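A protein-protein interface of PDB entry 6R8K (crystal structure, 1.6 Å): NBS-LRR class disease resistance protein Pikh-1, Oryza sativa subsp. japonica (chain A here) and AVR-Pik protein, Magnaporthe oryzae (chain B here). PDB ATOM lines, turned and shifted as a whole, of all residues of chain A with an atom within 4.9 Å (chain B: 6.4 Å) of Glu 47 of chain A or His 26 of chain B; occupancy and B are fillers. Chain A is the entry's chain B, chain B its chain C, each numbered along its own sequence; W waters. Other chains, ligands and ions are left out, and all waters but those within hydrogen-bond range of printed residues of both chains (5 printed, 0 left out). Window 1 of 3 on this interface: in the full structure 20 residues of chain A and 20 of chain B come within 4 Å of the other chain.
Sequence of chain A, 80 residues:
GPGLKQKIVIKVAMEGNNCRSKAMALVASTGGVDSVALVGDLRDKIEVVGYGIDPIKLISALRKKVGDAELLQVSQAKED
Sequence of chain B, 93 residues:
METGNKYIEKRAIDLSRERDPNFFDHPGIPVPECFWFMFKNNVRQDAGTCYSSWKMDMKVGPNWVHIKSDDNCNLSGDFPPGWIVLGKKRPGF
The side-chain hydroxyl (OG) of Ser 35 of chain A lies within hydrogen-bond range of a ring nitrogen (ND1) of His 26 of chain B. OE1 of Glu 47 of chain A is in hydrogen-bond range of NE2 of His 26 of chain B (2.7 Å).
O of Ser 35 of chain A sits at hydrogen-bond distance from N of Val 49 of chain A (3.0 Å). N of Glu 47 of chain A sits at hydrogen-bond distance from O of Ala 37 of chain A (2.9 Å).
Among the printed residues, merely in contact across the chains: Lys 7 of chain A with Thr 49 of chain B (3.97 Å), Ser 35 of chain A with Pro 27 of chain B (3.8 Å), Ala 37 of chain A with Phe 24 of chain B (3.4 Å), Glu 47 of chain A with Phe 24 of chain B (3.8 Å), Val 49 of chain A with His 26 of chain B (3.4 Å) and Val 49 of chain A with Ile 29 of chain B (3.8 Å).
Printed residues of chain B within 4 Å of Ser 35 of chain A: His 26 (2.8 Å) and Pro 27 (3.8 Å). Of the printed residues of chain B, Ala 37 of chain A touches Phe 24 (3.4 Å). Lys 45 of chain A touches none of the printed residues of chain B. Of chain B, only Phe 24 and His 26 come within 4 Å of Glu 47 of chain A. Of the printed residues of chain A, Phe 24 of chain B touches Ala 37 (3.4 Å) and Glu 47 (3.8 Å). Of chain A, only Ser 35, Glu 47 and Val 49 come within 4 Å of His 26 of chain B. Of the printed residues of chain A, Ile 29 of chain B touches Val 49. The nearest residue of chain A that does not touch His 26 of chain B is Ala 37 of chain A (4.1 Å).
Of the 12 printed residues of chain A, 5 touch a printed residue of chain B. Hydrophobic or aromatic side chains of chain A within 4 Å of the printed part of chain B: Ala 37 and Val 49. Hydrophobic or aromatic side chains of chain B within 4 Å of the printed part of chain A: Phe 24, His 26, Pro 27 and Ile 29. Along chain B the printed residues that touch a printed residue of chain A span positions 24 to 49. Among the printed residues, 8 pairs touch across the chains. Among the printed residues, no Asp or Glu carboxylate lies within 4 Å of a Lys or Arg side-chain nitrogen of the other chain.
Water W2 lies within hydrogen-bond range of NZ of Lys 7 of chain A (2.7 Å) and O of Thr 49 of chain B (2.9 Å). Water W4 lies within hydrogen-bond range of the side-chain carboxylate (OE1) of Glu 47 of chain A, the backbone NH (N) of Phe 24 of chain B and the side-chain hydroxyl (OG1) of Thr 49 of chain B. Water W3 lies within hydrogen-bond range of N of Gly 28 of chain B (2.8 Å) and OG of Ser 35 of chain A (2.9 Å). Water W5 lies within hydrogen-bond range of the side-chain hydroxyl (OG1) of Thr 49 of chain B (2.8 Å), the side-chain carboxylate (OE2) of Glu 47 of chain A (3.0 Å) and the side-chain amino group (NZ) of Lys 7 of chain A (3.0 Å). Water W1 bridges the backbone NH of Thr 49 of chain B and the side-chain carboxylate of Glu 47 of chain A.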
ATOM      1  N   LYS A   7     -11.920  14.138  -6.956  1.00  0.00           N
ATOM      2  CA  LYS A   7     -10.814  13.702  -6.089  1.00  0.00           C
ATOM      3  C   LYS A   7     -10.375  12.360  -6.640  1.00  0.00           C
ATOM      4  O   LYS A   7     -11.264  11.480  -6.837  1.00  0.00           O
ATOM      5  CB  LYS A   7     -11.265  13.603  -4.633  1.00  0.00           C
ATOM      6  CG  LYS A   7     -10.196  13.127  -3.652  1.00  0.00           C
ATOM      7  CD  LYS A   7     -10.594  13.241  -2.179  1.00  0.00           C
ATOM      8  CE  LYS A   7     -12.093  13.173  -1.937  1.00  0.00           C
ATOM      9  NZ  LYS A   7     -12.452  12.990  -0.508  1.00  0.00           N
ATOM     10  N   ILE A   8      -9.089  12.238  -6.918  1.00  0.00           N
ATOM     11  CA  ILE A   8      -8.516  11.033  -7.579  1.00  0.00           C
ATOM     12  C   ILE A   8      -7.411  10.518  -6.667  1.00  0.00           C
ATOM     13  O   ILE A   8      -6.601  11.319  -6.203  1.00  0.00           O
ATOM     14  CB  ILE A   8      -8.020  11.382  -9.001  1.00  0.00           C
ATOM     15  CG1 ILE A   8      -9.205  11.669  -9.931  1.00  0.00           C
ATOM     16  CG2 ILE A   8      -7.138  10.294  -9.582  1.00  0.00           C
ATOM     17  CD1 ILE A   8      -8.826  12.437 -11.175  1.00  0.00           C
ATOM     18  N   VAL A   9      -7.419   9.232  -6.312  1.00  0.00           N
ATOM     19  CA  VAL A   9      -6.300   8.688  -5.502  1.00  0.00           C
ATOM     20  C   VAL A   9      -5.553   7.637  -6.319  1.00  0.00           C
ATOM     21  O   VAL A   9      -6.215   6.704  -6.859  1.00  0.00           O
ATOM     22  CB  VAL A   9      -6.775   8.070  -4.174  1.00  0.00           C
ATOM     23  CG1 VAL A   9      -5.590   7.530  -3.401  1.00  0.00           C
ATOM     24  CG2 VAL A   9      -7.553   9.057  -3.326  1.00  0.00           C
ATOM     25  N   SER A  35      -4.950  20.837  -5.964  1.00  0.00           N
ATOM     26  CA  SER A  35      -4.241  20.451  -4.719  1.00  0.00           C
ATOM     27  C   SER A  35      -3.823  18.987  -4.798  1.00  0.00           C
ATOM     28  O   SER A  35      -4.475  18.219  -5.544  1.00  0.00           O
ATOM     29  CB  SER A  35      -5.047  20.721  -3.482  1.00  0.00           C
ATOM     30  OG  SER A  35      -6.357  20.185  -3.550  1.00  0.00           O
ATOM     31  N   VAL A  36      -2.699  18.675  -4.170  1.00  0.00           N
ATOM     32  CA  VAL A  36      -2.122  17.309  -4.151  1.00  0.00           C
ATOM     33  C   VAL A  36      -1.601  17.019  -2.742  1.00  0.00           C
ATOM     34  O   VAL A  36      -1.153  17.944  -2.071  1.00  0.00           O
ATOM     35  CB  VAL A  36      -1.063  17.146  -5.244  1.00  0.00           C
ATOM     36  CG1 VAL A  36       0.037  18.175  -5.122  1.00  0.00           C
ATOM     37  CG2 VAL A  36      -0.504  15.738  -5.251  1.00  0.00           C
ATOM     38  N   ALA A  37      -1.745  15.780  -2.273  1.00  0.00           N
ATOM     39  CA  ALA A  37      -1.240  15.392  -0.942  1.00  0.00           C
ATOM     40  C   ALA A  37      -0.830  13.923  -1.002  1.00  0.00           C
ATOM     41  O   ALA A  37      -1.378  13.145  -1.795  1.00  0.00           O
ATOM     42  CB  ALA A  37      -2.267  15.665   0.127  1.00  0.00           C
ATOM     43  N   VAL A  39      -0.934  10.631   1.135  1.00  0.00           N
ATOM     44  CA  VAL A  39      -1.851  10.138   2.189  1.00  0.00           C
ATOM     45  C   VAL A  39      -1.717   8.619   2.305  1.00  0.00           C
ATOM     46  O   VAL A  39      -0.956   7.989   1.566  1.00  0.00           O
ATOM     47  CB  VAL A  39      -3.298  10.576   1.880  1.00  0.00           C
ATOM     48  CG1 VAL A  39      -3.414  12.093   1.776  1.00  0.00           C
ATOM     49  CG2 VAL A  39      -3.800   9.924   0.614  1.00  0.00           C
ATOM     50  N   LYS A  45       0.115   6.835  -1.307  1.00  0.00           N
ATOM     51  CA  LYS A  45      -1.016   7.245  -2.160  1.00  0.00           C
ATOM     52  C   LYS A  45      -0.974   8.746  -2.413  1.00  0.00           C
ATOM     53  O   LYS A  45      -0.787   9.533  -1.466  1.00  0.00           O
ATOM     54  CB  LYS A  45      -2.336   6.807  -1.532  1.00  0.00           C
ATOM     55  CG  LYS A  45      -2.493   5.299  -1.695  1.00  0.00           C
ATOM     56  CD  LYS A  45      -3.464   4.659  -0.792  1.00  0.00           C
ATOM     57  CE  LYS A  45      -3.217   3.167  -0.681  1.00  0.00           C
ATOM     58  NZ  LYS A  45      -4.399   2.514  -0.071  1.00  0.00           N
ATOM     59  N   ILE A  46      -1.138   9.099  -3.670  1.00  0.00           N
ATOM     60  CA  ILE A  46      -1.248  10.516  -4.096  1.00  0.00           C
ATOM     61  C   ILE A  46      -2.722  10.830  -4.307  1.00  0.00           C
ATOM     62  O   ILE A  46      -3.356  10.215  -5.147  1.00  0.00           O
ATOM     63  CB  ILE A  46      -0.413  10.789  -5.365  1.00  0.00           C
ATOM     64  CG1 ILE A  46       1.043  10.361  -5.157  1.00  0.00           C
ATOM     65  CG2 ILE A  46      -0.512  12.258  -5.733  1.00  0.00           C
ATOM     66  CD1 ILE A  46       1.908  10.552  -6.376  1.00  0.00           C
ATOM     67  N   GLU A  47      -3.219  11.814  -3.570  1.00  0.00           N
ATOM     68  CA  GLU A  47      -4.605  12.308  -3.668  1.00  0.00           C
ATOM     69  C   GLU A  47      -4.587  13.635  -4.421  1.00  0.00           C
ATOM     70  O   GLU A  47      -3.847  14.519  -4.003  1.00  0.00           O
ATOM     71  CB  GLU A  47      -5.141  12.440  -2.250  1.00  0.00           C
ATOM     72  CG  GLU A  47      -6.624  12.622  -2.155  1.00  0.00           C
ATOM     73  CD  GLU A  47      -7.025  12.470  -0.697  1.00  0.00           C
ATOM     74  OE1 GLU A  47      -6.871  13.449   0.036  1.00  0.00           O
ATOM     75  OE2 GLU A  47      -7.332  11.325  -0.262  1.00  0.00           O
ATOM     76  N   VAL A  48      -5.319  13.696  -5.513  1.00  0.00           N
ATOM     77  CA  VAL A  48      -5.348  14.867  -6.441  1.00  0.00           C
ATOM     78  C   VAL A  48      -6.759  15.430  -6.471  1.00  0.00           C
ATOM     79  O   VAL A  48      -7.709  14.665  -6.634  1.00  0.00           O
ATOM     80  CB  VAL A  48      -4.891  14.421  -7.839  1.00  0.00           C
ATOM     81  CG1 VAL A  48      -4.552  15.634  -8.695  1.00  0.00           C
ATOM     82  CG2 VAL A  48      -3.721  13.459  -7.741  1.00  0.00           C
ATOM     83  N   VAL A  49      -6.916  16.748  -6.353  1.00  0.00           N
ATOM     84  CA  VAL A  49      -8.248  17.411  -6.422  1.00  0.00           C
ATOM     85  C   VAL A  49      -8.193  18.449  -7.543  1.00  0.00           C
ATOM     86  O   VAL A  49      -7.170  19.139  -7.641  1.00  0.00           O
ATOM     87  CB  VAL A  49      -8.609  18.056  -5.077  1.00  0.00           C
ATOM     88  CG1 VAL A  49      -9.839  18.936  -5.182  1.00  0.00           C
ATOM     89  CG2 VAL A  49      -8.781  16.992  -3.988  1.00  0.00           C
ATOM     90  N   PHE B  23      -4.443  11.876   6.512  1.00  0.00           N
ATOM     91  CA  PHE B  23      -5.325  12.551   5.536  1.00  0.00           C
ATOM     92  C   PHE B  23      -4.862  13.987   5.328  1.00  0.00           C
ATOM     93  O   PHE B  23      -4.047  14.514   6.103  1.00  0.00           O
ATOM     94  CB  PHE B  23      -6.772  12.490   6.017  1.00  0.00           C
ATOM     95  CG  PHE B  23      -7.021  13.310   7.250  1.00  0.00           C
ATOM     96  CD1 PHE B  23      -6.722  12.813   8.507  1.00  0.00           C
ATOM     97  CD2 PHE B  23      -7.559  14.583   7.153  1.00  0.00           C
ATOM     98  CE1 PHE B  23      -6.948  13.575   9.644  1.00  0.00           C
ATOM     99  CE2 PHE B  23      -7.764  15.352   8.289  1.00  0.00           C
ATOM    100  CZ  PHE B  23      -7.466  14.845   9.527  1.00  0.00           C
ATOM    101  N   PHE B  24      -5.472  14.643   4.348  1.00  0.00           N
ATOM    102  CA  PHE B  24      -5.233  16.074   4.036  1.00  0.00           C
ATOM    103  C   PHE B  24      -6.550  16.728   3.634  1.00  0.00           C
ATOM    104  O   PHE B  24      -7.177  16.235   2.675  1.00  0.00           O
ATOM    105  CB  PHE B  24      -4.227  16.224   2.904  1.00  0.00           C
ATOM    106  CG  PHE B  24      -3.974  17.664   2.538  1.00  0.00           C
ATOM    107  CD1 PHE B  24      -3.505  18.555   3.491  1.00  0.00           C
ATOM    108  CD2 PHE B  24      -4.244  18.132   1.272  1.00  0.00           C
ATOM    109  CE1 PHE B  24      -3.304  19.886   3.168  1.00  0.00           C
ATOM    110  CE2 PHE B  24      -4.021  19.457   0.946  1.00  0.00           C
ATOM    111  CZ  PHE B  24      -3.546  20.326   1.892  1.00  0.00           C
ATOM    112  N   ASP B  25      -6.995  17.765   4.355  1.00  0.00           N
ATOM    113  CA  ASP B  25      -8.219  18.506   3.981  1.00  0.00           C
ATOM    114  C   ASP B  25      -7.827  19.525   2.900  1.00  0.00           C
ATOM    115  O   ASP B  25      -7.388  20.646   3.217  1.00  0.00           O
ATOM    116  CB  ASP B  25      -8.947  19.094   5.190  1.00  0.00           C
ATOM    117  CG  ASP B  25      -9.516  18.048   6.150  1.00  0.00           C
ATOM    118  OD1 ASP B  25      -9.925  16.956   5.692  1.00  0.00           O
ATOM    119  OD2 ASP B  25      -9.534  18.336   7.362  1.00  0.00           O
ATOM    120  N   HIS B  26      -8.055  19.147   1.654  1.00  0.00           N
ATOM    121  CA  HIS B  26      -7.770  19.962   0.455  1.00  0.00           C
ATOM    122  C   HIS B  26      -8.448  21.323   0.579  1.00  0.00           C
ATOM    123  O   HIS B  26      -9.600  21.436   1.010  1.00  0.00           O
ATOM    124  CB  HIS B  26      -8.231  19.212  -0.785  1.00  0.00           C
ATOM    125  CG  HIS B  26      -7.424  17.980  -1.017  1.00  0.00           C
ATOM    126  ND1 HIS B  26      -6.259  17.969  -1.761  1.00  0.00           N
ATOM    127  CD2 HIS B  26      -7.584  16.724  -0.530  1.00  0.00           C
ATOM    128  CE1 HIS B  26      -5.763  16.739  -1.777  1.00  0.00           C
ATOM    129  NE2 HIS B  26      -6.561  15.954  -1.028  1.00  0.00           N
ATOM    130  N   PRO B  27      -7.708  22.398   0.215  1.00  0.00           N
ATOM    131  CA  PRO B  27      -8.179  23.766   0.481  1.00  0.00           C
ATOM    132  C   PRO B  27      -9.360  24.298  -0.357  1.00  0.00           C
ATOM    133  O   PRO B  27     -10.061  25.209   0.105  1.00  0.00           O
ATOM    134  CB  PRO B  27      -6.895  24.575   0.267  1.00  0.00           C
ATOM    135  CG  PRO B  27      -6.103  23.759  -0.716  1.00  0.00           C
ATOM    136  CD  PRO B  27      -6.328  22.332  -0.277  1.00  0.00           C
ATOM    137  N   GLY B  28      -9.585  23.739  -1.538  1.00  0.00           N
ATOM    138  CA  GLY B  28     -10.570  24.281  -2.492  1.00  0.00           C
ATOM    139  C   GLY B  28     -11.874  23.523  -2.484  1.00  0.00           C
ATOM    140  O   GLY B  28     -12.726  23.860  -3.334  1.00  0.00           O
ATOM    141  N   ILE B  29     -12.034  22.517  -1.613  1.00  0.00           N
ATOM    142  CA  ILE B  29     -13.301  21.737  -1.521  1.00  0.00           C
ATOM    143  C   ILE B  29     -13.760  21.653  -0.070  1.00  0.00           C
ATOM    144  O   ILE B  29     -12.975  21.822   0.869  1.00  0.00           O
ATOM    145  CB  ILE B  29     -13.149  20.340  -2.150  1.00  0.00           C
ATOM    146  CG1 ILE B  29     -11.963  19.603  -1.532  1.00  0.00           C
ATOM    147  CG2 ILE B  29     -13.047  20.414  -3.666  1.00  0.00           C
ATOM    148  CD1 ILE B  29     -11.902  18.143  -1.895  1.00  0.00           C
ATOM    149  N   PRO B  30     -15.055  21.395   0.171  1.00  0.00           N
ATOM    150  CA  PRO B  30     -15.549  21.292   1.530  1.00  0.00           C
ATOM    151  C   PRO B  30     -14.779  20.206   2.281  1.00  0.00           C
ATOM    152  O   PRO B  30     -14.300  19.245   1.687  1.00  0.00           O
ATOM    153  CB  PRO B  30     -17.031  20.961   1.352  1.00  0.00           C
ATOM    154  CG  PRO B  30     -17.341  21.623   0.049  1.00  0.00           C
ATOM    155  CD  PRO B  30     -16.147  21.271  -0.812  1.00  0.00           C
ATOM    156  N   VAL B  31     -14.637  20.429   3.581  1.00  0.00           N
ATOM    157  CA  VAL B  31     -14.021  19.433   4.487  1.00  0.00           C
ATOM    158  C   VAL B  31     -14.943  18.218   4.588  1.00  0.00           C
ATOM    159  O   VAL B  31     -16.101  18.342   4.970  1.00  0.00           O
ATOM    160  CB  VAL B  31     -13.721  20.046   5.864  1.00  0.00           C
ATOM    161  CG1 VAL B  31     -13.117  18.985   6.768  1.00  0.00           C
ATOM    162  CG2 VAL B  31     -12.800  21.252   5.754  1.00  0.00           C
ATOM    163  N   PRO B  32     -14.459  16.996   4.240  1.00  0.00           N
ATOM    164  CA  PRO B  32     -15.291  15.791   4.313  1.00  0.00           C
ATOM    165  C   PRO B  32     -15.562  15.394   5.762  1.00  0.00           C
ATOM    166  O   PRO B  32     -14.658  15.565   6.603  1.00  0.00           O
ATOM    167  CB  PRO B  32     -14.470  14.714   3.578  1.00  0.00           C
ATOM    168  CG  PRO B  32     -13.044  15.199   3.665  1.00  0.00           C
ATOM    169  CD  PRO B  32     -13.113  16.719   3.708  1.00  0.00           C
ATOM    170  N   GLY B  48      -8.971   6.632   5.205  1.00  0.00           N
ATOM    171  CA  GLY B  48      -8.953   7.994   4.648  1.00  0.00           C
ATOM    172  C   GLY B  48     -10.186   8.768   5.040  1.00  0.00           C
ATOM    173  O   GLY B  48     -10.865   8.409   6.005  1.00  0.00           O
ATOM    174  N   THR B  49     -10.488   9.817   4.286  1.00  0.00           N
ATOM    175  CA  THR B  49     -11.674  10.661   4.530  1.00  0.00           C
ATOM    176  C   THR B  49     -12.676  10.495   3.392  1.00  0.00           C
ATOM    177  O   THR B  49     -12.259  10.170   2.278  1.00  0.00           O
ATOM    178  CB  THR B  49     -11.301  12.137   4.697  1.00  0.00           C
ATOM    179  OG1 THR B  49     -10.639  12.561   3.512  1.00  0.00           O
ATOM    180  CG2 THR B  49     -10.461  12.434   5.919  1.00  0.00           C
HETATM  181  O   HOH W   1      -7.734  10.437   2.835  1.00  0.00           O
HETATM  182  O   HOH W   2     -13.270  10.441  -0.428  1.00  0.00           O
HETATM  183  O   HOH W   3      -8.691  21.857  -3.371  1.00  0.00           O
HETATM  184  O   HOH W   4      -7.363  13.187   2.682  1.00  0.00           O
HETATM  185  O   HOH W   5     -10.008  11.868   0.886  1.00  0.00           O
